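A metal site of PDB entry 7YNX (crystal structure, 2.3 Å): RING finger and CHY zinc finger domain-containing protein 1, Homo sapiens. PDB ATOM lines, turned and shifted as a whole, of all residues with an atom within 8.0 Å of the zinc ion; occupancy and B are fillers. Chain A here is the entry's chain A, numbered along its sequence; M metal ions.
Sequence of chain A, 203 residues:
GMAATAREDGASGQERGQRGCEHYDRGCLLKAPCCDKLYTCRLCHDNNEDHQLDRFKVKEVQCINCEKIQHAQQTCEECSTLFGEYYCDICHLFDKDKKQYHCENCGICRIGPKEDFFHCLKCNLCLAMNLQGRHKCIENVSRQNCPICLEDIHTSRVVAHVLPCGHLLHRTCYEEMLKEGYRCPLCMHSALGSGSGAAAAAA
N of Cys 146 lies within hydrogen-bond range of O of Glu 151 (2.8 Å).
The backbone NH (N) of Ile 148 sits close to the side-chain sulfur (SG) of Cys 146 (3.3 Å).
The side-chain sulfur of Cys 149 lies close to the backbone NH of Glu 151 (3.4 Å).
O of Asp 152 is in hydrogen-bond range of NE2 of His 170, 2.8 Å away.
Of the 18 residues printed, 4 come within 4 Å of the zinc ion.
The nearest printed residue that does not touch the zinc ion is Ile 148 (4.5 Å).
The zinc ion is bound by a ring nitrogen (ND1) of His 170 (2.1 Å), the side-chain sulfur of Cys 173 (2.4 Å), the side-chain sulfur of Cys 146 (2.4 Å) and the side-chain sulfur of Cys 149 (2.5 Å).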
ATOM      1  N   ASN A 145       1.626  -8.718   3.712  1.00  0.00           N
ATOM      2  CA  ASN A 145       1.949  -9.524   4.864  1.00  0.00           C
ATOM      3  C   ASN A 145       0.774 -10.437   5.201  1.00  0.00           C
ATOM      4  O   ASN A 145      -0.397 -10.114   4.951  1.00  0.00           O
ATOM      5  CB  ASN A 145       2.304  -8.621   6.055  1.00  0.00           C
ATOM      6  CG  ASN A 145       3.629  -7.885   5.860  1.00  0.00           C
ATOM      7  OD1 ASN A 145       4.504  -8.360   5.144  1.00  0.00           O
ATOM      8  ND2 ASN A 145       3.771  -6.721   6.497  1.00  0.00           N
ATOM      9  N   CYS A 146       1.089 -11.610   5.694  1.00  0.00           N
ATOM     10  CA  CYS A 146       0.097 -12.475   6.272  1.00  0.00           C
ATOM     11  C   CYS A 146      -0.622 -11.757   7.412  1.00  0.00           C
ATOM     12  O   CYS A 146       0.069 -11.261   8.328  1.00  0.00           O
ATOM     13  CB  CYS A 146       0.758 -13.749   6.781  1.00  0.00           C
ATOM     14  SG  CYS A 146      -0.318 -14.761   7.789  1.00  0.00           S
ATOM     15  N   PRO A 147      -1.933 -11.684   7.440  1.00  0.00           N
ATOM     16  CA  PRO A 147      -2.613 -10.958   8.520  1.00  0.00           C
ATOM     17  C   PRO A 147      -2.386 -11.571   9.898  1.00  0.00           C
ATOM     18  O   PRO A 147      -2.595 -10.889  10.905  1.00  0.00           O
ATOM     19  CB  PRO A 147      -4.099 -10.984   8.128  1.00  0.00           C
ATOM     20  CG  PRO A 147      -4.212 -12.075   7.159  1.00  0.00           C
ATOM     21  CD  PRO A 147      -2.900 -12.152   6.418  1.00  0.00           C
ATOM     22  N   ILE A 148      -1.959 -12.836   9.978  1.00  0.00           N
ATOM     23  CA  ILE A 148      -1.704 -13.478  11.271  1.00  0.00           C
ATOM     24  C   ILE A 148      -0.348 -13.015  11.787  1.00  0.00           C
ATOM     25  O   ILE A 148      -0.259 -12.351  12.825  1.00  0.00           O
ATOM     26  CB  ILE A 148      -1.731 -15.013  11.165  1.00  0.00           C
ATOM     27  CG1 ILE A 148      -3.074 -15.500  10.606  1.00  0.00           C
ATOM     28  CG2 ILE A 148      -1.438 -15.648  12.521  1.00  0.00           C
ATOM     29  CD1 ILE A 148      -4.113 -15.737  11.642  1.00  0.00           C
ATOM     30  N   CYS A 149       0.718 -13.395  11.083  1.00  0.00           N
ATOM     31  CA  CYS A 149       2.070 -13.106  11.543  1.00  0.00           C
ATOM     32  C   CYS A 149       2.603 -11.775  11.062  1.00  0.00           C
ATOM     33  O   CYS A 149       3.621 -11.318  11.581  1.00  0.00           O
ATOM     34  CB  CYS A 149       3.021 -14.212  11.101  1.00  0.00           C
ATOM     35  SG  CYS A 149       3.279 -14.239   9.313  1.00  0.00           S
ATOM     36  N   LEU A 150       1.948 -11.154  10.075  1.00  0.00           N
ATOM     37  CA  LEU A 150       2.368  -9.872   9.512  1.00  0.00           C
ATOM     38  C   LEU A 150       3.803  -9.932   8.975  1.00  0.00           C
ATOM     39  O   LEU A 150       4.578  -8.979   9.067  1.00  0.00           O
ATOM     40  CB  LEU A 150       2.187  -8.727  10.532  1.00  0.00           C
ATOM     41  CG  LEU A 150       0.729  -8.373  10.893  1.00  0.00           C
ATOM     42  CD1 LEU A 150       0.664  -7.392  12.052  1.00  0.00           C
ATOM     43  CD2 LEU A 150      -0.065  -7.842   9.716  1.00  0.00           C
ATOM     44  N   GLU A 151       4.159 -11.082   8.399  1.00  0.00           N
ATOM     45  CA  GLU A 151       5.347 -11.228   7.577  1.00  0.00           C
ATOM     46  C   GLU A 151       4.935 -11.590   6.153  1.00  0.00           C
ATOM     47  O   GLU A 151       3.845 -12.129   5.916  1.00  0.00           O
ATOM     48  CB  GLU A 151       6.308 -12.269   8.144  1.00  0.00           C
ATOM     49  CG  GLU A 151       7.348 -11.670   9.082  1.00  0.00           C
ATOM     50  CD  GLU A 151       7.695 -12.570  10.238  1.00  0.00           C
ATOM     51  OE1 GLU A 151       7.895 -12.040  11.356  1.00  0.00           O
ATOM     52  OE2 GLU A 151       7.750 -13.809  10.022  1.00  0.00           O
ATOM     53  N   ASP A 152       5.819 -11.286   5.211  1.00  0.00           N
ATOM     54  CA  ASP A 152       5.487 -11.381   3.794  1.00  0.00           C
ATOM     55  C   ASP A 152       5.010 -12.792   3.389  1.00  0.00           C
ATOM     56  O   ASP A 152       5.499 -13.816   3.879  1.00  0.00           O
ATOM     57  CB  ASP A 152       6.699 -10.976   2.949  1.00  0.00           C
ATOM     58  CG  ASP A 152       6.341 -10.744   1.475  1.00  0.00           C
ATOM     59  OD1 ASP A 152       5.376 -10.004   1.194  1.00  0.00           O
ATOM     60  OD2 ASP A 152       7.037 -11.291   0.602  1.00  0.00           O
ATOM     61  N   ILE A 153       4.039 -12.812   2.481  1.00  0.00           N
ATOM     62  CA  ILE A 153       3.522 -14.036   1.887  1.00  0.00           C
ATOM     63  C   ILE A 153       4.318 -14.408   0.648  1.00  0.00           C
ATOM     64  O   ILE A 153       4.670 -15.572   0.460  1.00  0.00           O
ATOM     65  CB  ILE A 153       2.038 -13.854   1.524  1.00  0.00           C
ATOM     66  CG1 ILE A 153       1.169 -13.772   2.770  1.00  0.00           C
ATOM     67  CG2 ILE A 153       1.599 -14.927   0.537  1.00  0.00           C
ATOM     68  CD1 ILE A 153       0.140 -12.665   2.691  1.00  0.00           C
ATOM     69  N   SER A 156       7.803 -15.976   0.916  1.00  0.00           N
ATOM     70  CA  SER A 156       7.960 -16.913   2.015  1.00  0.00           C
ATOM     71  C   SER A 156       8.162 -18.325   1.488  1.00  0.00           C
ATOM     72  O   SER A 156       7.537 -18.712   0.497  1.00  0.00           O
ATOM     73  CB  SER A 156       6.750 -16.874   2.936  1.00  0.00           C
ATOM     74  OG  SER A 156       6.791 -17.954   3.847  1.00  0.00           O
ATOM     75  N   VAL A 158       7.176 -20.856   3.097  1.00  0.00           N
ATOM     76  CA  VAL A 158       6.001 -21.610   3.510  1.00  0.00           C
ATOM     77  C   VAL A 158       4.926 -21.442   2.441  1.00  0.00           C
ATOM     78  O   VAL A 158       4.664 -20.327   1.969  1.00  0.00           O
ATOM     79  CB  VAL A 158       5.508 -21.141   4.889  1.00  0.00           C
ATOM     80  CG1 VAL A 158       4.259 -21.940   5.305  1.00  0.00           C
ATOM     81  CG2 VAL A 158       6.617 -21.304   5.911  1.00  0.00           C
ATOM     82  N   LEU A 168      -4.966 -14.506   1.715  1.00  0.00           N
ATOM     83  CA  LEU A 168      -3.865 -15.471   1.757  1.00  0.00           C
ATOM     84  C   LEU A 168      -3.258 -15.536   3.154  1.00  0.00           C
ATOM     85  O   LEU A 168      -3.008 -14.487   3.764  1.00  0.00           O
ATOM     86  CB  LEU A 168      -2.784 -15.108   0.740  1.00  0.00           C
ATOM     87  CG  LEU A 168      -3.057 -15.370  -0.737  1.00  0.00           C
ATOM     88  CD1 LEU A 168      -2.045 -14.639  -1.617  1.00  0.00           C
ATOM     89  CD2 LEU A 168      -3.029 -16.861  -1.015  1.00  0.00           C
ATOM     90  N   LEU A 169      -3.008 -16.751   3.623  1.00  0.00           N
ATOM     91  CA  LEU A 169      -2.344 -17.004   4.902  1.00  0.00           C
ATOM     92  C   LEU A 169      -1.222 -18.006   4.672  1.00  0.00           C
ATOM     93  O   LEU A 169      -1.319 -18.858   3.789  1.00  0.00           O
ATOM     94  CB  LEU A 169      -3.323 -17.583   5.953  1.00  0.00           C
ATOM     95  CG  LEU A 169      -4.601 -16.808   6.274  1.00  0.00           C
ATOM     96  CD1 LEU A 169      -5.443 -17.566   7.240  1.00  0.00           C
ATOM     97  CD2 LEU A 169      -4.228 -15.471   6.865  1.00  0.00           C
ATOM     98  N   HIS A 170      -0.159 -17.903   5.467  1.00  0.00           N
ATOM     99  CA  HIS A 170       0.815 -18.982   5.520  1.00  0.00           C
ATOM    100  C   HIS A 170       0.130 -20.267   5.978  1.00  0.00           C
ATOM    101  O   HIS A 170      -0.756 -20.242   6.842  1.00  0.00           O
ATOM    102  CB  HIS A 170       1.965 -18.625   6.461  1.00  0.00           C
ATOM    103  CG  HIS A 170       2.751 -17.414   6.033  1.00  0.00           C
ATOM    104  ND1 HIS A 170       3.078 -16.392   6.893  1.00  0.00           N
ATOM    105  CD2 HIS A 170       3.258 -17.069   4.832  1.00  0.00           C
ATOM    106  CE1 HIS A 170       3.755 -15.471   6.244  1.00  0.00           C
ATOM    107  NE2 HIS A 170       3.886 -15.861   4.985  1.00  0.00           N
ATOM    108  N   ARG A 171       0.489 -21.391   5.361  1.00  0.00           N
ATOM    109  CA  ARG A 171      -0.112 -22.662   5.762  1.00  0.00           C
ATOM    110  C   ARG A 171       0.025 -22.881   7.258  1.00  0.00           C
ATOM    111  O   ARG A 171      -0.932 -23.278   7.936  1.00  0.00           O
ATOM    112  CB  ARG A 171       0.520 -23.822   4.994  1.00  0.00           C
ATOM    113  CG  ARG A 171      -0.395 -25.038   4.834  1.00  0.00           C
ATOM    114  CD  ARG A 171       0.020 -25.875   3.627  1.00  0.00           C
ATOM    115  NE  ARG A 171       1.064 -26.827   3.986  1.00  0.00           N
ATOM    116  CZ  ARG A 171       1.870 -27.444   3.117  1.00  0.00           C
ATOM    117  NH1 ARG A 171       1.775 -27.210   1.816  1.00  0.00           N
ATOM    118  NH2 ARG A 171       2.784 -28.297   3.553  1.00  0.00           N
ATOM    119  N   THR A 172       1.200 -22.584   7.809  1.00  0.00           N
ATOM    120  CA  THR A 172       1.440 -22.739   9.240  1.00  0.00           C
ATOM    121  C   THR A 172       0.524 -21.840  10.058  1.00  0.00           C
ATOM    122  O   THR A 172      -0.063 -22.267  11.055  1.00  0.00           O
ATOM    123  CB  THR A 172       2.907 -22.442   9.539  1.00  0.00           C
ATOM    124  OG1 THR A 172       3.257 -21.200   8.943  1.00  0.00           O
ATOM    125  CG2 THR A 172       3.789 -23.527   8.942  1.00  0.00           C
ATOM    126  N   CYS A 173       0.397 -20.566   9.669  1.00  0.00           N
ATOM    127  CA  CYS A 173      -0.475 -19.669  10.412  1.00  0.00           C
ATOM    128  C   CYS A 173      -1.928 -20.050  10.245  1.00  0.00           C
ATOM    129  O   CYS A 173      -2.722 -19.869  11.167  1.00  0.00           O
ATOM    130  CB  CYS A 173      -0.280 -18.232   9.935  1.00  0.00           C
ATOM    131  SG  CYS A 173       1.413 -17.738  10.051  1.00  0.00           S
ATOM    132  N   TYR A 174      -2.274 -20.571   9.071  1.00  0.00           N
ATOM    133  CA  TYR A 174      -3.645 -20.984   8.817  1.00  0.00           C
ATOM    134  C   TYR A 174      -4.032 -22.143   9.724  1.00  0.00           C
ATOM    135  O   TYR A 174      -5.115 -22.139  10.316  1.00  0.00           O
ATOM    136  CB  TYR A 174      -3.770 -21.361   7.352  1.00  0.00           C
ATOM    137  CG  TYR A 174      -5.006 -22.101   6.984  1.00  0.00           C
ATOM    138  CD1 TYR A 174      -6.264 -21.514   7.080  1.00  0.00           C
ATOM    139  CD2 TYR A 174      -4.932 -23.410   6.512  1.00  0.00           C
ATOM    140  CE1 TYR A 174      -7.403 -22.214   6.733  1.00  0.00           C
ATOM    141  CE2 TYR A 174      -6.057 -24.099   6.149  1.00  0.00           C
ATOM    142  CZ  TYR A 174      -7.284 -23.507   6.266  1.00  0.00           C
ATOM    143  OH  TYR A 174      -8.383 -24.235   5.885  1.00  0.00           O
HETATM  144 ZN    ZN M   1       1.709 -15.957   8.442  1.00  0.00          ZN
